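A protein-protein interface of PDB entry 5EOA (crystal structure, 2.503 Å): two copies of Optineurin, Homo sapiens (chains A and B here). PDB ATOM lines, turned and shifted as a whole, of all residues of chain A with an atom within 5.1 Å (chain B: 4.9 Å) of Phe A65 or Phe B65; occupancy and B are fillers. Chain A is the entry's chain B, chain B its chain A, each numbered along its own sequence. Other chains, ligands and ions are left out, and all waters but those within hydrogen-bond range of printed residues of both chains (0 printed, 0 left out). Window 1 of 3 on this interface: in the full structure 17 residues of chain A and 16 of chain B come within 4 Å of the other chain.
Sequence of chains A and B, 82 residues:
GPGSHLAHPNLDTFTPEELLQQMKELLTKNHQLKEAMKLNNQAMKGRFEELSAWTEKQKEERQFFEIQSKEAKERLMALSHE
The guanidinium group (NE) of Arg A62 lies within salt-bridge range of the side-chain carboxylate (OE1) of Glu B61 (2.8 Å). The guanidinium group of Arg B62 is in salt-bridge range of the side-chain carboxylate of Glu A61. The side-chain amide oxygen (OE1) of Gln A68 is in hydrogen-bond range of the side-chain hydroxyl (OG) of Ser B69 (3.3 Å).
OE1 of Glu B66 lies within salt-bridge range of NE of Arg B62, at 3.4 Å. The side-chain carboxylate (OE2) of Glu A66 lies within salt-bridge range of the guanidinium group (NH1) of Arg A62 (2.6 Å).
Phe B65 touches Arg A62. CE2 of Phe A65 touches NH2 of Arg B62, at 3.3 Å. Phe B65 touches Phe A65. Glu B66 touches Phe A65 (CG to CE1, 3.6 Å). Glu A66 touches Phe B65 (CG to CZ, 3.7 Å). Ser A69 touches Phe B65. Ser A69 touches Gln B68. Ser A69 touches Ser B69 (N to OG, 3.6 Å).
Of chain A, only Arg A62 (3.6 Å), Phe A65 (3.5 Å), Glu A66 (3.7 Å) and Ser A69 (3.7 Å) come within 4 Å of Phe B65. Of the printed residues of chain B, Arg A62 touches Glu B61 (2.8 Å) and Phe B65 (3.6 Å). Of the printed residues of chain B, Ser A69 touches Phe B65, Gln B68 and Ser B69. Lys A70 touches none of the printed residues of chain B. Phe B64 touches none of the printed residues of chain A. The nearest printed residue of chain B that does not touch Phe A65 is Ser B69 (5.0 Å). The nearest printed residue of chain A that does not touch Phe B65 is Gln A68 (5.8 Å). The nearest printed residue of chain A that does not touch Ser B69 is Phe A65 (5.0 Å).
Of the 10 printed residues of chain A, 6 touch a printed residue of chain B. Printed residues of chain A that touch a printed residue of chain B: Glu A61, Arg A62, Phe A65, Glu A66, Gln A68 and Ser A69. Hydrophobic or aromatic side chains of chain A within 4 Å of the printed part of chain B: Phe A65. Printed residues of chain B that touch a printed residue of chain A: Glu B61, Arg B62, Phe B65, Glu B66, Gln B68 and Ser B69. Among the printed residues, 11 pairs touch across the chains. Among the printed residues, Asp or Glu carboxylates within 4 Å of a Lys or Arg side-chain nitrogen of the other chain: Glu A61 with Arg B62 and Arg A62 with Glu B61.
Glu A61 touches Arg B62, and with the chains exchanged Arg A62 touches Glu B61. Arg A62 touches Phe B65, and with the chains exchanged Phe A65 touches Arg B62. Phe A65 touches Glu B66, and with the chains exchanged Glu A66 touches Phe B65. Gln A68 touches Ser B69, and with the chains exchanged Ser A69 touches Gln B68. 9 positions are printed for both chains.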
ATOM      1  N   GLU A  61      21.300  -1.270  -1.724  1.00  0.00           N
ATOM      2  CA  GLU A  61      21.073  -2.069  -2.924  1.00  0.00           C
ATOM      3  C   GLU A  61      21.173  -3.578  -2.672  1.00  0.00           C
ATOM      4  O   GLU A  61      20.411  -4.361  -3.232  1.00  0.00           O
ATOM      5  CB  GLU A  61      22.011  -1.622  -4.055  1.00  0.00           C
ATOM      6  CG  GLU A  61      21.699  -0.202  -4.559  1.00  0.00           C
ATOM      7  CD  GLU A  61      22.533   0.231  -5.766  1.00  0.00           C
ATOM      8  OE1 GLU A  61      23.522  -0.459  -6.111  1.00  0.00           O
ATOM      9  OE2 GLU A  61      22.191   1.273  -6.371  1.00  0.00           O
ATOM     10  N   ARG A  62      22.106  -3.976  -1.822  1.00  0.00           N
ATOM     11  CA  ARG A  62      22.263  -5.373  -1.448  1.00  0.00           C
ATOM     12  C   ARG A  62      21.078  -5.804  -0.579  1.00  0.00           C
ATOM     13  O   ARG A  62      20.464  -6.846  -0.802  1.00  0.00           O
ATOM     14  CB  ARG A  62      23.564  -5.531  -0.668  1.00  0.00           C
ATOM     15  CG  ARG A  62      23.917  -6.953  -0.336  1.00  0.00           C
ATOM     16  CD  ARG A  62      25.081  -6.994   0.629  1.00  0.00           C
ATOM     17  NE  ARG A  62      25.263  -8.336   1.154  1.00  0.00           N
ATOM     18  CZ  ARG A  62      24.441  -8.893   2.035  1.00  0.00           C
ATOM     19  NH1 ARG A  62      23.386  -8.214   2.481  1.00  0.00           N
ATOM     20  NH2 ARG A  62      24.665 -10.128   2.467  1.00  0.00           N
ATOM     21  N   GLN A  63      20.773  -4.974   0.412  1.00  0.00           N
ATOM     22  CA  GLN A  63      19.650  -5.175   1.303  1.00  0.00           C
ATOM     23  C   GLN A  63      18.354  -5.433   0.534  1.00  0.00           C
ATOM     24  O   GLN A  63      17.542  -6.269   0.936  1.00  0.00           O
ATOM     25  CB  GLN A  63      19.482  -3.931   2.179  1.00  0.00           C
ATOM     26  CG  GLN A  63      19.898  -4.114   3.622  1.00  0.00           C
ATOM     27  CD  GLN A  63      18.737  -4.513   4.507  1.00  0.00           C
ATOM     28  OE1 GLN A  63      18.075  -3.657   5.103  1.00  0.00           O
ATOM     29  NE2 GLN A  63      18.478  -5.817   4.597  1.00  0.00           N
ATOM     30  N   PHE A  64      18.167  -4.702  -0.561  1.00  0.00           N
ATOM     31  CA  PHE A  64      16.961  -4.804  -1.349  1.00  0.00           C
ATOM     32  C   PHE A  64      16.860  -6.189  -1.982  1.00  0.00           C
ATOM     33  O   PHE A  64      15.873  -6.917  -1.788  1.00  0.00           O
ATOM     34  CB  PHE A  64      16.948  -3.731  -2.429  1.00  0.00           C
ATOM     35  CG  PHE A  64      15.801  -3.861  -3.386  1.00  0.00           C
ATOM     36  CD1 PHE A  64      14.538  -3.390  -3.046  1.00  0.00           C
ATOM     37  CD2 PHE A  64      15.980  -4.461  -4.628  1.00  0.00           C
ATOM     38  CE1 PHE A  64      13.476  -3.521  -3.923  1.00  0.00           C
ATOM     39  CE2 PHE A  64      14.915  -4.589  -5.506  1.00  0.00           C
ATOM     40  CZ  PHE A  64      13.664  -4.114  -5.149  1.00  0.00           C
ATOM     41  N   PHE A  65      17.893  -6.556  -2.732  1.00  0.00           N
ATOM     42  CA  PHE A  65      17.914  -7.859  -3.366  1.00  0.00           C
ATOM     43  C   PHE A  65      17.956  -8.998  -2.366  1.00  0.00           C
ATOM     44  O   PHE A  65      17.441 -10.083  -2.643  1.00  0.00           O
ATOM     45  CB  PHE A  65      19.064  -7.943  -4.360  1.00  0.00           C
ATOM     46  CG  PHE A  65      18.866  -7.060  -5.537  1.00  0.00           C
ATOM     47  CD1 PHE A  65      17.865  -7.333  -6.446  1.00  0.00           C
ATOM     48  CD2 PHE A  65      19.646  -5.937  -5.718  1.00  0.00           C
ATOM     49  CE1 PHE A  65      17.656  -6.514  -7.531  1.00  0.00           C
ATOM     50  CE2 PHE A  65      19.440  -5.116  -6.798  1.00  0.00           C
ATOM     51  CZ  PHE A  65      18.441  -5.409  -7.711  1.00  0.00           C
ATOM     52  N   GLU A  66      18.572  -8.759  -1.213  1.00  0.00           N
ATOM     53  CA  GLU A  66      18.600  -9.773  -0.176  1.00  0.00           C
ATOM     54  C   GLU A  66      17.179 -10.054   0.338  1.00  0.00           C
ATOM     55  O   GLU A  66      16.796 -11.211   0.511  1.00  0.00           O
ATOM     56  CB  GLU A  66      19.502  -9.351   0.971  1.00  0.00           C
ATOM     57  CG  GLU A  66      19.582 -10.376   2.080  1.00  0.00           C
ATOM     58  CD  GLU A  66      20.454  -9.932   3.239  1.00  0.00           C
ATOM     59  OE1 GLU A  66      20.608 -10.720   4.191  1.00  0.00           O
ATOM     60  OE2 GLU A  66      20.989  -8.804   3.206  1.00  0.00           O
ATOM     61  N   ILE A  67      16.400  -8.998   0.565  1.00  0.00           N
ATOM     62  CA  ILE A  67      15.041  -9.152   1.062  1.00  0.00           C
ATOM     63  C   ILE A  67      14.131  -9.724  -0.021  1.00  0.00           C
ATOM     64  O   ILE A  67      13.274 -10.557   0.261  1.00  0.00           O
ATOM     65  CB  ILE A  67      14.476  -7.825   1.588  1.00  0.00           C
ATOM     66  CG1 ILE A  67      15.239  -7.394   2.835  1.00  0.00           C
ATOM     67  CG2 ILE A  67      12.999  -7.942   1.945  1.00  0.00           C
ATOM     68  CD1 ILE A  67      14.879  -5.980   3.312  1.00  0.00           C
ATOM     69  N   GLN A  68      14.334  -9.275  -1.253  1.00  0.00           N
ATOM     70  CA  GLN A  68      13.569  -9.742  -2.388  1.00  0.00           C
ATOM     71  C   GLN A  68      13.756 -11.239  -2.507  1.00  0.00           C
ATOM     72  O   GLN A  68      12.797 -11.987  -2.660  1.00  0.00           O
ATOM     73  CB  GLN A  68      14.055  -9.072  -3.663  1.00  0.00           C
ATOM     74  CG  GLN A  68      12.978  -8.340  -4.421  1.00  0.00           C
ATOM     75  CD  GLN A  68      13.315  -8.248  -5.887  1.00  0.00           C
ATOM     76  OE1 GLN A  68      14.297  -8.840  -6.339  1.00  0.00           O
ATOM     77  NE2 GLN A  68      12.503  -7.512  -6.643  1.00  0.00           N
ATOM     78  N   SER A  69      15.006 -11.667  -2.418  1.00  0.00           N
ATOM     79  CA  SER A  69      15.345 -13.076  -2.481  1.00  0.00           C
ATOM     80  C   SER A  69      14.665 -13.866  -1.363  1.00  0.00           C
ATOM     81  O   SER A  69      14.124 -14.939  -1.592  1.00  0.00           O
ATOM     82  CB  SER A  69      16.862 -13.232  -2.378  1.00  0.00           C
ATOM     83  OG  SER A  69      17.232 -14.592  -2.354  1.00  0.00           O
ATOM     84  N   LYS A  70      14.704 -13.325  -0.154  1.00  0.00           N
ATOM     85  CA  LYS A  70      14.170 -13.997   1.011  1.00  0.00           C
ATOM     86  C   LYS A  70      12.668 -14.218   0.848  1.00  0.00           C
ATOM     87  O   LYS A  70      12.156 -15.329   1.059  1.00  0.00           O
ATOM     88  CB  LYS A  70      14.453 -13.154   2.249  1.00  0.00           C
ATOM     89  CG  LYS A  70      13.988 -13.754   3.561  1.00  0.00           C
ATOM     90  CD  LYS A  70      13.751 -12.669   4.609  1.00  0.00           C
ATOM     91  CE  LYS A  70      12.605 -11.747   4.188  1.00  0.00           C
ATOM     92  NZ  LYS A  70      12.409 -10.560   5.084  1.00  0.00           N
ATOM     93  N   GLU B  61      27.742 -10.369  -4.085  1.00  0.00           N
ATOM     94  CA  GLU B  61      26.651 -10.804  -3.238  1.00  0.00           C
ATOM     95  C   GLU B  61      25.314 -10.294  -3.765  1.00  0.00           C
ATOM     96  O   GLU B  61      24.297 -10.987  -3.683  1.00  0.00           O
ATOM     97  CB  GLU B  61      26.898 -10.368  -1.794  1.00  0.00           C
ATOM     98  CG  GLU B  61      28.139 -11.025  -1.210  1.00  0.00           C
ATOM     99  CD  GLU B  61      28.331 -10.739   0.263  1.00  0.00           C
ATOM    100  OE1 GLU B  61      27.612  -9.866   0.803  1.00  0.00           O
ATOM    101  OE2 GLU B  61      29.203 -11.395   0.876  1.00  0.00           O
ATOM    102  N   ARG B  62      25.321  -9.093  -4.333  1.00  0.00           N
ATOM    103  CA  ARG B  62      24.094  -8.495  -4.833  1.00  0.00           C
ATOM    104  C   ARG B  62      23.542  -9.300  -5.998  1.00  0.00           C
ATOM    105  O   ARG B  62      22.413  -9.799  -5.954  1.00  0.00           O
ATOM    106  CB  ARG B  62      24.338  -7.063  -5.280  1.00  0.00           C
ATOM    107  CG  ARG B  62      23.181  -6.463  -6.049  1.00  0.00           C
ATOM    108  CD  ARG B  62      23.614  -6.032  -7.437  1.00  0.00           C
ATOM    109  NE  ARG B  62      22.606  -5.191  -8.079  1.00  0.00           N
ATOM    110  CZ  ARG B  62      22.454  -3.891  -7.834  1.00  0.00           C
ATOM    111  NH1 ARG B  62      23.239  -3.282  -6.951  1.00  0.00           N
ATOM    112  NH2 ARG B  62      21.514  -3.196  -8.468  1.00  0.00           N
ATOM    113  N   GLN B  63      24.349  -9.445  -7.036  1.00  0.00           N
ATOM    114  CA  GLN B  63      23.890 -10.160  -8.202  1.00  0.00           C
ATOM    115  C   GLN B  63      23.711 -11.646  -7.897  1.00  0.00           C
ATOM    116  O   GLN B  63      23.051 -12.346  -8.656  1.00  0.00           O
ATOM    117  CB  GLN B  63      24.826  -9.941  -9.383  1.00  0.00           C
ATOM    118  CG  GLN B  63      26.015 -10.850  -9.385  1.00  0.00           C
ATOM    119  CD  GLN B  63      26.801 -10.750 -10.671  1.00  0.00           C
ATOM    120  OE1 GLN B  63      27.437  -9.727 -10.947  1.00  0.00           O
ATOM    121  NE2 GLN B  63      26.760 -11.813 -11.471  1.00  0.00           N
ATOM    122  N   PHE B  64      24.274 -12.132  -6.792  1.00  0.00           N
ATOM    123  CA  PHE B  64      23.928 -13.474  -6.337  1.00  0.00           C
ATOM    124  C   PHE B  64      22.459 -13.494  -5.901  1.00  0.00           C
ATOM    125  O   PHE B  64      21.670 -14.338  -6.346  1.00  0.00           O
ATOM    126  CB  PHE B  64      24.833 -13.936  -5.197  1.00  0.00           C
ATOM    127  CG  PHE B  64      24.355 -15.193  -4.512  1.00  0.00           C
ATOM    128  CD1 PHE B  64      24.572 -16.441  -5.083  1.00  0.00           C
ATOM    129  CD2 PHE B  64      23.693 -15.126  -3.291  1.00  0.00           C
ATOM    130  CE1 PHE B  64      24.130 -17.597  -4.455  1.00  0.00           C
ATOM    131  CE2 PHE B  64      23.258 -16.275  -2.659  1.00  0.00           C
ATOM    132  CZ  PHE B  64      23.481 -17.510  -3.242  1.00  0.00           C
ATOM    133  N   PHE B  65      22.104 -12.548  -5.038  1.00  0.00           N
ATOM    134  CA  PHE B  65      20.741 -12.417  -4.537  1.00  0.00           C
ATOM    135  C   PHE B  65      19.738 -12.182  -5.649  1.00  0.00           C
ATOM    136  O   PHE B  65      18.603 -12.661  -5.591  1.00  0.00           O
ATOM    137  CB  PHE B  65      20.664 -11.255  -3.555  1.00  0.00           C
ATOM    138  CG  PHE B  65      21.234 -11.571  -2.208  1.00  0.00           C
ATOM    139  CD1 PHE B  65      20.862 -12.727  -1.541  1.00  0.00           C
ATOM    140  CD2 PHE B  65      22.146 -10.724  -1.611  1.00  0.00           C
ATOM    141  CE1 PHE B  65      21.396 -13.023  -0.303  1.00  0.00           C
ATOM    142  CE2 PHE B  65      22.674 -11.016  -0.381  1.00  0.00           C
ATOM    143  CZ  PHE B  65      22.297 -12.173   0.274  1.00  0.00           C
ATOM    144  N   GLU B  66      20.165 -11.424  -6.651  1.00  0.00           N
ATOM    145  CA  GLU B  66      19.298 -11.036  -7.739  1.00  0.00           C
ATOM    146  C   GLU B  66      19.021 -12.283  -8.570  1.00  0.00           C
ATOM    147  O   GLU B  66      17.876 -12.540  -8.963  1.00  0.00           O
ATOM    148  CB  GLU B  66      19.974  -9.946  -8.562  1.00  0.00           C
ATOM    149  CG  GLU B  66      19.064  -9.184  -9.512  1.00  0.00           C
ATOM    150  CD  GLU B  66      19.784  -8.033 -10.224  1.00  0.00           C
ATOM    151  OE1 GLU B  66      20.908  -7.640  -9.805  1.00  0.00           O
ATOM    152  OE2 GLU B  66      19.212  -7.523 -11.212  1.00  0.00           O
ATOM    153  N   ILE B  67      20.067 -13.074  -8.803  1.00  0.00           N
ATOM    154  CA  ILE B  67      19.923 -14.351  -9.496  1.00  0.00           C
ATOM    155  C   ILE B  67      19.034 -15.302  -8.704  1.00  0.00           C
ATOM    156  O   ILE B  67      18.153 -15.951  -9.276  1.00  0.00           O
ATOM    157  CB  ILE B  67      21.293 -15.008  -9.764  1.00  0.00           C
ATOM    158  CG1 ILE B  67      21.893 -14.455 -11.051  1.00  0.00           C
ATOM    159  CG2 ILE B  67      21.175 -16.524  -9.869  1.00  0.00           C
ATOM    160  CD1 ILE B  67      23.286 -14.961 -11.331  1.00  0.00           C
ATOM    161  N   GLN B  68      19.260 -15.384  -7.395  1.00  0.00           N
ATOM    162  CA  GLN B  68      18.465 -16.275  -6.554  1.00  0.00           C
ATOM    163  C   GLN B  68      16.993 -15.880  -6.558  1.00  0.00           C
ATOM    164  O   GLN B  68      16.107 -16.739  -6.492  1.00  0.00           O
ATOM    165  CB  GLN B  68      19.008 -16.323  -5.126  1.00  0.00           C
ATOM    166  CG  GLN B  68      20.174 -17.271  -4.949  1.00  0.00           C
ATOM    167  CD  GLN B  68      19.954 -18.247  -3.810  1.00  0.00           C
ATOM    168  OE1 GLN B  68      19.360 -17.895  -2.788  1.00  0.00           O
ATOM    169  NE2 GLN B  68      20.426 -19.486  -3.980  1.00  0.00           N
ATOM    170  N   SER B  69      16.740 -14.582  -6.667  1.00  0.00           N
ATOM    171  CA  SER B  69      15.381 -14.062  -6.632  1.00  0.00           C
ATOM    172  C   SER B  69      14.633 -14.439  -7.899  1.00  0.00           C
ATOM    173  O   SER B  69      13.490 -14.880  -7.845  1.00  0.00           O
ATOM    174  CB  SER B  69      15.400 -12.543  -6.482  1.00  0.00           C
ATOM    175  OG  SER B  69      14.195 -12.079  -5.905  1.00  0.00           O
